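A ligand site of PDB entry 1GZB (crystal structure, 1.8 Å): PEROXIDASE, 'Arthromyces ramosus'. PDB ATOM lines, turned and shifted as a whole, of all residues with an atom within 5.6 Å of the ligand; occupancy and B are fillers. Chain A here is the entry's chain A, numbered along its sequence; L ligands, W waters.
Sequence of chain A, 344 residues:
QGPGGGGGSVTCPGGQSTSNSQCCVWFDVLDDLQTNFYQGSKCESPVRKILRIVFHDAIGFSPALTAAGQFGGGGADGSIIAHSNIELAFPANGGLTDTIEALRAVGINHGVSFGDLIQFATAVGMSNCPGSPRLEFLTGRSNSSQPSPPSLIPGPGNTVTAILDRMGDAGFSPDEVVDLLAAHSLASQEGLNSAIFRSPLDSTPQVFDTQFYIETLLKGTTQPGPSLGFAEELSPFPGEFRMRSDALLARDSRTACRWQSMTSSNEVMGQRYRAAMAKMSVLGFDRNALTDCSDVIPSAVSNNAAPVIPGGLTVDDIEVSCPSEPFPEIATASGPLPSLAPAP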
ATOM      1  N   SER A  45      30.601 -24.378  16.481  1.00  0.00           N
ATOM      2  CA  SER A  45      31.092 -24.908  17.744  1.00  0.00           C
ATOM      3  C   SER A  45      32.426 -24.307  18.277  1.00  0.00           C
ATOM      4  O   SER A  45      32.437 -23.982  19.469  1.00  0.00           O
ATOM      5  CB  SER A  45      31.202 -26.441  17.557  1.00  0.00           C
ATOM      6  OG  SER A  45      31.361 -27.084  18.809  1.00  0.00           O
ATOM      7  N   VAL A  47      33.663 -21.247  18.162  1.00  0.00           N
ATOM      8  CA  VAL A  47      33.414 -19.951  18.800  1.00  0.00           C
ATOM      9  C   VAL A  47      32.707 -20.158  20.135  1.00  0.00           C
ATOM     10  O   VAL A  47      33.003 -19.500  21.117  1.00  0.00           O
ATOM     11  CB  VAL A  47      32.514 -19.047  17.952  1.00  0.00           C
ATOM     12  CG1 VAL A  47      32.259 -17.716  18.643  1.00  0.00           C
ATOM     13  CG2 VAL A  47      33.197 -18.799  16.625  1.00  0.00           C
ATOM     14  N   ARG A  48      31.799 -21.115  20.184  1.00  0.00           N
ATOM     15  CA  ARG A  48      31.026 -21.394  21.373  1.00  0.00           C
ATOM     16  C   ARG A  48      31.837 -21.939  22.531  1.00  0.00           C
ATOM     17  O   ARG A  48      31.720 -21.502  23.673  1.00  0.00           O
ATOM     18  CB  ARG A  48      29.903 -22.352  21.001  1.00  0.00           C
ATOM     19  CG  ARG A  48      28.963 -21.787  19.974  1.00  0.00           C
ATOM     20  CD  ARG A  48      27.790 -22.653  20.123  1.00  0.00           C
ATOM     21  NE  ARG A  48      27.423 -22.955  18.811  1.00  0.00           N
ATOM     22  CZ  ARG A  48      27.406 -24.134  18.255  1.00  0.00           C
ATOM     23  NH1 ARG A  48      27.721 -25.288  18.804  1.00  0.00           N
ATOM     24  NH2 ARG A  48      27.075 -24.077  16.999  1.00  0.00           N
ATOM     25  N   LYS A  49      32.738 -22.863  22.212  1.00  0.00           N
ATOM     26  CA  LYS A  49      33.626 -23.469  23.168  1.00  0.00           C
ATOM     27  C   LYS A  49      34.581 -22.377  23.635  1.00  0.00           C
ATOM     28  O   LYS A  49      34.802 -22.292  24.839  1.00  0.00           O
ATOM     29  CB  LYS A  49      34.444 -24.619  22.554  1.00  0.00           C
ATOM     30  CG  LYS A  49      33.728 -25.798  21.913  1.00  0.00           C
ATOM     31  CD  LYS A  49      33.031 -26.546  23.010  1.00  0.00           C
ATOM     32  CE  LYS A  49      32.688 -27.929  22.639  1.00  0.00           C
ATOM     33  NZ  LYS A  49      32.065 -28.548  23.812  1.00  0.00           N
ATOM     34  N   LEU A  51      34.074 -19.152  24.021  1.00  0.00           N
ATOM     35  CA  LEU A  51      33.361 -18.272  24.943  1.00  0.00           C
ATOM     36  C   LEU A  51      33.212 -18.930  26.325  1.00  0.00           C
ATOM     37  O   LEU A  51      33.261 -18.218  27.326  1.00  0.00           O
ATOM     38  CB  LEU A  51      31.990 -17.895  24.306  1.00  0.00           C
ATOM     39  CG  LEU A  51      32.011 -16.822  23.141  1.00  0.00           C
ATOM     40  CD1 LEU A  51      30.678 -16.715  22.429  1.00  0.00           C
ATOM     41  CD2 LEU A  51      32.261 -15.449  23.734  1.00  0.00           C
ATOM     42  N   ARG A  52      33.035 -20.270  26.460  1.00  0.00           N
ATOM     43  CA  ARG A  52      32.980 -20.923  27.769  1.00  0.00           C
ATOM     44  C   ARG A  52      34.398 -20.848  28.331  1.00  0.00           C
ATOM     45  O   ARG A  52      34.573 -20.561  29.517  1.00  0.00           O
ATOM     46  CB  ARG A  52      32.702 -22.399  27.784  1.00  0.00           C
ATOM     47  CG  ARG A  52      31.309 -22.834  27.485  1.00  0.00           C
ATOM     48  CD  ARG A  52      31.216 -24.358  27.333  1.00  0.00           C
ATOM     49  NE  ARG A  52      31.451 -25.066  28.583  1.00  0.00           N
ATOM     50  CZ  ARG A  52      31.752 -26.382  28.607  1.00  0.00           C
ATOM     51  NH1 ARG A  52      31.841 -27.099  27.473  1.00  0.00           N
ATOM     52  NH2 ARG A  52      32.002 -26.976  29.781  1.00  0.00           N
ATOM     53  N   VAL A  54      36.969 -18.526  27.799  1.00  0.00           N
ATOM     54  CA  VAL A  54      37.402 -17.228  28.292  1.00  0.00           C
ATOM     55  C   VAL A  54      36.771 -16.926  29.662  1.00  0.00           C
ATOM     56  O   VAL A  54      37.438 -16.439  30.582  1.00  0.00           O
ATOM     57  CB  VAL A  54      37.042 -16.208  27.177  1.00  0.00           C
ATOM     58  CG1 VAL A  54      35.549 -15.898  27.152  1.00  0.00           C
ATOM     59  CG2 VAL A  54      37.832 -14.917  27.432  1.00  0.00           C
ATOM     60  N   PHE A  55      35.498 -17.346  29.847  1.00  0.00           N
ATOM     61  CA  PHE A  55      34.793 -17.150  31.081  1.00  0.00           C
ATOM     62  C   PHE A  55      35.475 -18.017  32.138  1.00  0.00           C
ATOM     63  O   PHE A  55      35.892 -17.482  33.149  1.00  0.00           O
ATOM     64  CB  PHE A  55      33.299 -17.568  30.937  1.00  0.00           C
ATOM     65  CG  PHE A  55      32.430 -17.494  32.216  1.00  0.00           C
ATOM     66  CD1 PHE A  55      32.570 -16.471  33.132  1.00  0.00           C
ATOM     67  CD2 PHE A  55      31.544 -18.520  32.516  1.00  0.00           C
ATOM     68  CE1 PHE A  55      31.846 -16.484  34.302  1.00  0.00           C
ATOM     69  CE2 PHE A  55      30.830 -18.533  33.687  1.00  0.00           C
ATOM     70  CZ  PHE A  55      30.981 -17.518  34.584  1.00  0.00           C
ATOM     71  N   PRO A 154      30.617 -20.743  38.602  1.00  0.00           N
ATOM     72  CA  PRO A 154      29.179 -20.893  38.824  1.00  0.00           C
ATOM     73  C   PRO A 154      28.654 -22.119  38.081  1.00  0.00           C
ATOM     74  O   PRO A 154      29.100 -22.428  36.963  1.00  0.00           O
ATOM     75  CB  PRO A 154      28.561 -19.624  38.291  1.00  0.00           C
ATOM     76  CG  PRO A 154      29.643 -18.616  38.448  1.00  0.00           C
ATOM     77  CD  PRO A 154      30.933 -19.386  38.146  1.00  0.00           C
ATOM     78  N   GLY A 155      27.727 -22.885  38.678  1.00  0.00           N
ATOM     79  CA  GLY A 155      27.181 -24.052  38.034  1.00  0.00           C
ATOM     80  C   GLY A 155      25.723 -23.817  37.706  1.00  0.00           C
ATOM     81  O   GLY A 155      25.062 -22.995  38.339  1.00  0.00           O
ATOM     82  N   PRO A 156      25.148 -24.536  36.754  1.00  0.00           N
ATOM     83  CA  PRO A 156      23.767 -24.408  36.315  1.00  0.00           C
ATOM     84  C   PRO A 156      22.704 -24.816  37.327  1.00  0.00           C
ATOM     85  O   PRO A 156      21.524 -24.438  37.188  1.00  0.00           O
ATOM     86  CB  PRO A 156      23.741 -25.214  35.047  1.00  0.00           C
ATOM     87  CG  PRO A 156      24.601 -26.383  35.415  1.00  0.00           C
ATOM     88  CD  PRO A 156      25.758 -25.710  36.135  1.00  0.00           C
ATOM     89  N   ILE A 163      25.206 -17.662  42.624  1.00  0.00           N
ATOM     90  CA  ILE A 163      25.774 -17.074  41.401  1.00  0.00           C
ATOM     91  C   ILE A 163      26.076 -15.594  41.644  1.00  0.00           C
ATOM     92  O   ILE A 163      27.185 -15.147  41.316  1.00  0.00           O
ATOM     93  CB  ILE A 163      24.745 -17.255  40.215  1.00  0.00           C
ATOM     94  CG1 ILE A 163      24.576 -18.724  39.916  1.00  0.00           C
ATOM     95  CG2 ILE A 163      25.238 -16.572  38.940  1.00  0.00           C
ATOM     96  CD1 ILE A 163      23.395 -19.073  38.980  1.00  0.00           C
ATOM     97  N   MET A 167      29.995 -14.188  41.550  1.00  0.00           N
ATOM     98  CA  MET A 167      30.250 -13.168  40.571  1.00  0.00           C
ATOM     99  C   MET A 167      30.559 -11.832  41.236  1.00  0.00           C
ATOM    100  O   MET A 167      31.471 -11.121  40.787  1.00  0.00           O
ATOM    101  CB  MET A 167      29.050 -13.042  39.631  1.00  0.00           C
ATOM    102  CG  MET A 167      28.782 -14.131  38.599  1.00  0.00           C
ATOM    103  SD  MET A 167      30.173 -14.590  37.534  1.00  0.00           S
ATOM    104  CE  MET A 167      29.758 -13.562  36.144  1.00  0.00           C
ATOM    105  N   VAL A 177      26.247  -9.425  35.562  1.00  0.00           N
ATOM    106  CA  VAL A 177      26.055 -10.862  35.429  1.00  0.00           C
ATOM    107  C   VAL A 177      25.042 -11.023  34.285  1.00  0.00           C
ATOM    108  O   VAL A 177      25.274 -11.810  33.375  1.00  0.00           O
ATOM    109  CB  VAL A 177      25.487 -11.510  36.744  1.00  0.00           C
ATOM    110  CG1 VAL A 177      25.201 -12.983  36.545  1.00  0.00           C
ATOM    111  CG2 VAL A 177      26.452 -11.261  37.883  1.00  0.00           C
ATOM    112  N   LEU A 180      26.699 -10.236  30.912  1.00  0.00           N
ATOM    113  CA  LEU A 180      27.637 -11.270  30.479  1.00  0.00           C
ATOM    114  C   LEU A 180      26.953 -12.468  29.836  1.00  0.00           C
ATOM    115  O   LEU A 180      27.494 -13.102  28.931  1.00  0.00           O
ATOM    116  CB  LEU A 180      28.418 -11.728  31.668  1.00  0.00           C
ATOM    117  CG  LEU A 180      29.904 -11.472  31.837  1.00  0.00           C
ATOM    118  CD1 LEU A 180      30.451 -10.464  30.873  1.00  0.00           C
ATOM    119  CD2 LEU A 180      30.076 -11.117  33.308  1.00  0.00           C
ATOM    120  N   LEU A 181      25.740 -12.730  30.300  1.00  0.00           N
ATOM    121  CA  LEU A 181      24.928 -13.822  29.793  1.00  0.00           C
ATOM    122  C   LEU A 181      24.432 -13.596  28.379  1.00  0.00           C
ATOM    123  O   LEU A 181      23.799 -14.503  27.814  1.00  0.00           O
ATOM    124  CB  LEU A 181      23.747 -14.058  30.699  1.00  0.00           C
ATOM    125  CG  LEU A 181      23.683 -15.277  31.621  1.00  0.00           C
ATOM    126  CD1 LEU A 181      24.772 -16.284  31.324  1.00  0.00           C
ATOM    127  CD2 LEU A 181      23.840 -14.816  33.036  1.00  0.00           C
ATOM    128  N   ALA A 183      26.181 -13.869  25.964  1.00  0.00           N
ATOM    129  CA  ALA A 183      26.883 -14.890  25.249  1.00  0.00           C
ATOM    130  C   ALA A 183      26.021 -16.160  25.151  1.00  0.00           C
ATOM    131  O   ALA A 183      26.276 -17.011  24.293  1.00  0.00           O
ATOM    132  CB  ALA A 183      28.179 -15.155  25.975  1.00  0.00           C
ATOM    133  N   HIS A 184      24.944 -16.346  25.930  1.00  0.00           N
ATOM    134  CA  HIS A 184      24.111 -17.527  25.724  1.00  0.00           C
ATOM    135  C   HIS A 184      23.211 -17.386  24.461  1.00  0.00           C
ATOM    136  O   HIS A 184      22.435 -18.276  24.077  1.00  0.00           O
ATOM    137  CB  HIS A 184      23.283 -17.782  26.970  1.00  0.00           C
ATOM    138  CG  HIS A 184      24.018 -18.577  28.058  1.00  0.00           C
ATOM    139  ND1 HIS A 184      23.392 -19.117  29.179  1.00  0.00           N
ATOM    140  CD2 HIS A 184      25.380 -18.903  28.097  1.00  0.00           C
ATOM    141  CE1 HIS A 184      24.332 -19.793  29.862  1.00  0.00           C
ATOM    142  NE2 HIS A 184      25.465 -19.682  29.266  1.00  0.00           N
ATOM    143  N   LEU A 186      24.664 -17.309  21.624  1.00  0.00           N
ATOM    144  CA  LEU A 186      25.477 -18.010  20.639  1.00  0.00           C
ATOM    145  C   LEU A 186      25.804 -19.315  21.362  1.00  0.00           C
ATOM    146  O   LEU A 186      26.965 -19.655  21.595  1.00  0.00           O
ATOM    147  CB  LEU A 186      26.702 -17.113  20.412  1.00  0.00           C
ATOM    148  CG  LEU A 186      26.986 -16.172  19.229  1.00  0.00           C
ATOM    149  CD1 LEU A 186      25.768 -15.998  18.340  1.00  0.00           C
ATOM    150  CD2 LEU A 186      27.609 -14.915  19.805  1.00  0.00           C
ATOM    151  N   ALA A 187      24.795 -20.097  21.691  1.00  0.00           N
ATOM    152  CA  ALA A 187      25.020 -21.237  22.546  1.00  0.00           C
ATOM    153  C   ALA A 187      24.187 -22.472  22.424  1.00  0.00           C
ATOM    154  O   ALA A 187      23.052 -22.405  21.974  1.00  0.00           O
ATOM    155  CB  ALA A 187      24.882 -20.753  23.981  1.00  0.00           C
ATOM    156  N   SER A 188      24.733 -23.568  22.890  1.00  0.00           N
ATOM    157  CA  SER A 188      24.044 -24.850  22.948  1.00  0.00           C
ATOM    158  C   SER A 188      24.656 -25.597  24.164  1.00  0.00           C
ATOM    159  O   SER A 188      25.499 -25.045  24.918  1.00  0.00           O
ATOM    160  CB  SER A 188      24.261 -25.648  21.646  1.00  0.00           C
ATOM    161  OG  SER A 188      25.533 -26.251  21.567  1.00  0.00           O
ATOM    162  N   GLN A 189      24.171 -26.818  24.422  1.00  0.00           N
ATOM    163  CA  GLN A 189      24.739 -27.631  25.472  1.00  0.00           C
ATOM    164  C   GLN A 189      25.062 -28.973  24.822  1.00  0.00           C
ATOM    165  O   GLN A 189      24.403 -29.400  23.861  1.00  0.00           O
ATOM    166  CB  GLN A 189      23.750 -27.836  26.644  1.00  0.00           C
ATOM    167  CG  GLN A 189      22.477 -28.601  26.311  1.00  0.00           C
ATOM    168  CD  GLN A 189      22.588 -30.125  26.274  1.00  0.00           C
ATOM    169  OE1 GLN A 189      23.473 -30.710  26.914  1.00  0.00           O
ATOM    170  NE2 GLN A 189      21.692 -30.760  25.518  1.00  0.00           N
ATOM    171  N   GLU A 190      26.024 -29.666  25.351  1.00  0.00           N
ATOM    172  CA  GLU A 190      26.416 -30.978  24.854  1.00  0.00           C
ATOM    173  C   GLU A 190      26.452 -31.986  25.994  1.00  0.00           C
ATOM    174  O   GLU A 190      26.295 -33.199  25.796  1.00  0.00           O
ATOM    175  CB  GLU A 190      27.809 -30.963  24.244  1.00  0.00           C
ATOM    176  CG  GLU A 190      27.918 -30.150  22.985  1.00  0.00           C
ATOM    177  CD  GLU A 190      29.301 -30.098  22.327  1.00  0.00           C
ATOM    178  OE1 GLU A 190      30.280 -30.634  22.840  1.00  0.00           O
ATOM    179  OE2 GLU A 190      29.425 -29.497  21.271  1.00  0.00           O
ATOM    180  N   GLY A 191      26.680 -31.531  27.237  1.00  0.00           N
ATOM    181  CA  GLY A 191      26.844 -32.476  28.336  1.00  0.00           C
ATOM    182  C   GLY A 191      25.818 -32.429  29.429  1.00  0.00           C
ATOM    183  O   GLY A 191      25.915 -33.196  30.390  1.00  0.00           O
ATOM    184  N   LEU A 192      24.827 -31.576  29.322  1.00  0.00           N
ATOM    185  CA  LEU A 192      23.776 -31.512  30.325  1.00  0.00           C
ATOM    186  C   LEU A 192      22.763 -32.596  29.968  1.00  0.00           C
ATOM    187  O   LEU A 192      22.323 -33.366  30.827  1.00  0.00           O
ATOM    188  CB  LEU A 192      23.216 -30.096  30.294  1.00  0.00           C
ATOM    189  CG  LEU A 192      23.435 -29.130  31.458  1.00  0.00           C
ATOM    190  CD1 LEU A 192      24.679 -29.453  32.279  1.00  0.00           C
ATOM    191  CD2 LEU A 192      23.465 -27.740  30.864  1.00  0.00           C
ATOM    192  N   LEU A 201      20.312 -22.743  22.860  1.00  0.00           N
ATOM    193  CA  LEU A 201      19.733 -22.063  24.006  1.00  0.00           C
ATOM    194  C   LEU A 201      18.831 -20.924  23.525  1.00  0.00           C
ATOM    195  O   LEU A 201      18.072 -20.356  24.315  1.00  0.00           O
ATOM    196  CB  LEU A 201      20.864 -21.579  24.895  1.00  0.00           C
ATOM    197  CG  LEU A 201      21.301 -22.474  26.059  1.00  0.00           C
ATOM    198  CD1 LEU A 201      21.264 -23.955  25.749  1.00  0.00           C
ATOM    199  CD2 LEU A 201      22.648 -21.949  26.495  1.00  0.00           C
ATOM    200  N   MET A 243      18.201 -24.031  30.592  1.00  0.00           N
ATOM    201  CA  MET A 243      19.054 -24.233  31.729  1.00  0.00           C
ATOM    202  C   MET A 243      18.419 -23.554  32.964  1.00  0.00           C
ATOM    203  O   MET A 243      17.974 -22.397  32.891  1.00  0.00           O
ATOM    204  CB  MET A 243      20.404 -23.631  31.344  1.00  0.00           C
ATOM    205  CG  MET A 243      21.569 -23.908  32.240  1.00  0.00           C
ATOM    206  SD  MET A 243      23.030 -22.923  31.813  1.00  0.00           S
ATOM    207  CE  MET A 243      23.075 -23.410  30.109  1.00  0.00           C
ATOM    208  N   SER A 245      19.719 -22.145  35.753  1.00  0.00           N
ATOM    209  CA  SER A 245      20.228 -20.857  36.174  1.00  0.00           C
ATOM    210  C   SER A 245      19.712 -19.707  35.290  1.00  0.00           C
ATOM    211  O   SER A 245      19.398 -18.628  35.820  1.00  0.00           O
ATOM    212  CB  SER A 245      21.764 -20.927  36.147  1.00  0.00           C
ATOM    213  OG  SER A 245      22.304 -21.461  34.939  1.00  0.00           O
ATOM    214  N   LEU A 249      17.468 -16.710  36.784  1.00  0.00           N
ATOM    215  CA  LEU A 249      17.922 -15.338  36.672  1.00  0.00           C
ATOM    216  C   LEU A 249      16.950 -14.474  35.909  1.00  0.00           C
ATOM    217  O   LEU A 249      16.853 -13.291  36.200  1.00  0.00           O
ATOM    218  CB  LEU A 249      19.267 -15.292  35.984  1.00  0.00           C
ATOM    219  CG  LEU A 249      20.443 -15.788  36.834  1.00  0.00           C
ATOM    220  CD1 LEU A 249      21.628 -16.065  35.928  1.00  0.00           C
ATOM    221  CD2 LEU A 249      20.785 -14.767  37.901  1.00  0.00           C
ATOM    222  N   TYR A 273      27.256  -5.760  26.777  1.00  0.00           N
ATOM    223  CA  TYR A 273      28.064  -6.960  26.724  1.00  0.00           C
ATOM    224  C   TYR A 273      29.535  -6.588  26.487  1.00  0.00           C
ATOM    225  O   TYR A 273      30.396  -7.072  27.221  1.00  0.00           O
ATOM    226  CB  TYR A 273      27.548  -7.900  25.608  1.00  0.00           C
ATOM    227  CG  TYR A 273      28.389  -9.150  25.413  1.00  0.00           C
ATOM    228  CD1 TYR A 273      28.400 -10.190  26.348  1.00  0.00           C
ATOM    229  CD2 TYR A 273      29.131  -9.246  24.270  1.00  0.00           C
ATOM    230  CE1 TYR A 273      29.154 -11.342  26.129  1.00  0.00           C
ATOM    231  CE2 TYR A 273      29.894 -10.377  24.042  1.00  0.00           C
ATOM    232  CZ  TYR A 273      29.894 -11.406  24.962  1.00  0.00           C
ATOM    233  OH  TYR A 273      30.602 -12.537  24.644  1.00  0.00           O
ATOM    234  N   MET A 277      32.550  -7.507  29.110  1.00  0.00           N
ATOM    235  CA  MET A 277      33.633  -8.333  28.650  1.00  0.00           C
ATOM    236  C   MET A 277      34.944  -7.621  28.749  1.00  0.00           C
ATOM    237  O   MET A 277      35.927  -8.281  29.048  1.00  0.00           O
ATOM    238  CB  MET A 277      33.474  -8.748  27.208  1.00  0.00           C
ATOM    239  CG  MET A 277      32.331  -9.746  27.060  1.00  0.00           C
ATOM    240  SD  MET A 277      32.726 -11.403  27.656  1.00  0.00           S
ATOM    241  CE  MET A 277      33.868 -11.867  26.397  1.00  0.00           C
ATOM    242  N   MET A 280      35.948  -8.166  32.181  1.00  0.00           N
ATOM    243  CA  MET A 280      36.325  -9.515  32.485  1.00  0.00           C
ATOM    244  C   MET A 280      37.716  -9.890  31.961  1.00  0.00           C
ATOM    245  O   MET A 280      38.456 -10.658  32.597  1.00  0.00           O
ATOM    246  CB  MET A 280      35.284 -10.463  31.903  1.00  0.00           C
ATOM    247  CG  MET A 280      35.497 -11.839  32.455  1.00  0.00           C
ATOM    248  SD  MET A 280      34.239 -13.069  32.046  1.00  0.00           S
ATOM    249  CE  MET A 280      34.687 -13.218  30.340  1.00  0.00           C
HETATM  250  C1  LIG L   1      27.178 -23.090  27.666  1.00  0.00           C
HETATM  251  C2  LIG L   1      26.536 -22.470  32.394  1.00  0.00           C
HETATM  252  C3  LIG L   1      27.811 -17.884  31.999  1.00  0.00           C
HETATM  253  C4  LIG L   1      29.255 -18.777  27.521  1.00  0.00           C
HETATM  254  C5  LIG L   1      26.935 -23.325  29.001  1.00  0.00           C
HETATM  255  C6  LIG L   1      26.707 -24.618  29.584  1.00  0.00           C
HETATM  256  C7  LIG L   1      26.583 -24.459  30.913  1.00  0.00           C
HETATM  257  C8  LIG L   1      26.710 -23.049  31.166  1.00  0.00           C
HETATM  258  C9  LIG L   1      26.299 -25.533  31.939  1.00  0.00           C
HETATM  259  C10 LIG L   1      26.563 -25.931  28.821  1.00  0.00           C
HETATM  260  C11 LIG L   1      27.866 -26.566  28.447  1.00  0.00           C
HETATM  261  C12 LIG L   1      27.678 -27.920  27.792  1.00  0.00           C
HETATM  262  O1  LIG L   1      28.013 -28.077  26.642  1.00  0.00           O
HETATM  263  O2  LIG L   1      27.158 -28.861  28.401  1.00  0.00           O
HETATM  264  C13 LIG L   1      26.637 -21.125  32.660  1.00  0.00           C
HETATM  265  C14 LIG L   1      26.457 -20.530  33.979  1.00  0.00           C
HETATM  266  C15 LIG L   1      26.806 -19.230  33.874  1.00  0.00           C
HETATM  267  C16 LIG L   1      27.154 -19.009  32.462  1.00  0.00           C
HETATM  268  C17 LIG L   1      25.976 -21.227  35.242  1.00  0.00           C
HETATM  269  C18 LIG L   1      26.947 -18.345  34.949  1.00  0.00           C
HETATM  270  C19 LIG L   1      25.956 -17.368  35.349  1.00  0.00           C
HETATM  271  C20 LIG L   1      28.388 -17.747  30.762  1.00  0.00           C
HETATM  272  C21 LIG L   1      29.283 -16.669  30.413  1.00  0.00           C
HETATM  273  C22 LIG L   1      29.794 -16.956  29.197  1.00  0.00           C
HETATM  274  C23 LIG L   1      29.161 -18.216  28.786  1.00  0.00           C
HETATM  275  C24 LIG L   1      29.549 -15.411  31.234  1.00  0.00           C
HETATM  276  C25 LIG L   1      30.777 -16.292  28.480  1.00  0.00           C
HETATM  277  C26 LIG L   1      30.820 -14.906  28.151  1.00  0.00           C
HETATM  278  C27 LIG L   1      28.605 -19.946  27.105  1.00  0.00           C
HETATM  279  C28 LIG L   1      28.526 -20.416  25.746  1.00  0.00           C
HETATM  280  C29 LIG L   1      27.984 -21.651  25.802  1.00  0.00           C
HETATM  281  C30 LIG L   1      27.639 -21.884  27.166  1.00  0.00           C
HETATM  282  C31 LIG L   1      28.821 -19.565  24.518  1.00  0.00           C
HETATM  283  C32 LIG L   1      27.722 -22.605  24.648  1.00  0.00           C
HETATM  284  C33 LIG L   1      28.733 -23.720  24.457  1.00  0.00           C
HETATM  285  C34 LIG L   1      28.480 -24.634  23.271  1.00  0.00           C
HETATM  286  O3  LIG L   1      29.253 -25.552  23.084  1.00  0.00           O
HETATM  287  O4  LIG L   1      27.544 -24.437  22.513  1.00  0.00           O
HETATM  288  N1  LIG L   1      26.975 -22.365  29.996  1.00  0.00           N
HETATM  289  N2  LIG L   1      27.026 -20.175  31.726  1.00  0.00           N
HETATM  290  N3  LIG L   1      28.327 -18.694  29.778  1.00  0.00           N
HETATM  291  N4  LIG L   1      27.952 -20.798  27.952  1.00  0.00           N
HETATM  292 FE1  LIG L   1      27.397 -20.448  29.807  1.00  0.00          FE
HETATM  293  O   HOH W   1      29.969 -26.933  25.291  1.00  0.00           O
HETATM  294  O   HOH W   2      29.415 -26.739  20.745  1.00  0.00           O
HETATM  295  O   HOH W   3      29.821 -22.075  32.382  1.00  0.00           O
HETATM  296  O   HOH W   4      29.037 -23.706  34.475  1.00  0.00           O
HETATM  297  O   HOH W   5      30.501 -29.849  26.877  1.00  0.00           O
HETATM  298  O   HOH W   6      28.103 -29.227  30.890  1.00  0.00           O
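An iron atom (FE1) of the ligand is bound by a ring nitrogen (NE2) of His 184. N of Glu 190 lies within hydrogen-bond range of O1 of the ligand (2.9 Å). O4 of the ligand lies within hydrogen-bond range of N of Ser 188 (3.0 Å). The side-chain hydroxyl (OG) of Ser 188 sits at hydrogen-bond distance from an oxygen (O4) of the ligand, 2.9 Å away. The backbone NH (N) of Gly 191 is in hydrogen-bond range of an oxygen (O2) of the ligand (3.0 Å). O4 of the ligand is in salt-bridge range of NH1 of Arg 48 (3.8 Å).
The side-chain carboxylate (OE1) of Glu 190 is in salt-bridge range of the side-chain amino group (NZ) of Lys 49 (2.9 Å). The side-chain amide oxygen (OE1) of Gln 189 is in hydrogen-bond range of the backbone NH (N) of Gly 191, at 3.3 Å. O of Ala 187 is in hydrogen-bond range of N of Leu 201. The side-chain amide oxygen of Gln 189 is in hydrogen-bond range of the backbone NH of Leu 192. SD of Met 243 lies within hydrogen-bond range of OG of Ser 245 (3.5 Å). The backbone NH (N) of Ser 245 is in hydrogen-bond range of the backbone carbonyl oxygen (O) of Pro 156.
Merely in contact with the ligand: Leu 51, Ala 183, Ala 187, Leu 186, Leu 181, Gln 189, Phe 55, Met 243, Gly 155, Ser 245, Leu 192, Pro 156, Ile 163, Pro 154, Arg 52, Leu 180 and Lys 49. Hydrophobic or aromatic side chains that line the ligand: Leu 51, Phe 55, Pro 154, Pro 156, Ile 163, Leu 180, Leu 181, Ala 183, His 184, Ala 187, Leu 192 and Met 243. 22 residues have an atom within 4 Å of the ligand: Arg 48, Lys 49, Leu 51, Arg 52, Phe 55, Pro 154, Gly 155, Pro 156, Ile 163, Leu 180, Leu 181, Ala 183, His 184, Leu 186, Ala 187, Ser 188, Gln 189, Glu 190, Gly 191, Leu 192, Met 243 and Ser 245. The nearest printed residue that does not touch the ligand is Met 277 (4.02 Å).
Water W2 lies within hydrogen-bond range of O3 of the ligand (2.6 Å), OG of Ser 45 (2.8 Å), OE2 of Glu 190 (2.8 Å) and NH1 of Arg 48 (3.0 Å). Water W1 lies within hydrogen-bond range of O1 of the ligand, NH1 of Arg 52 and NZ of Lys 49. Water W5 bridges O1 of the ligand (3.1 Å) and NH1 of Arg 52 (3.1 Å).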
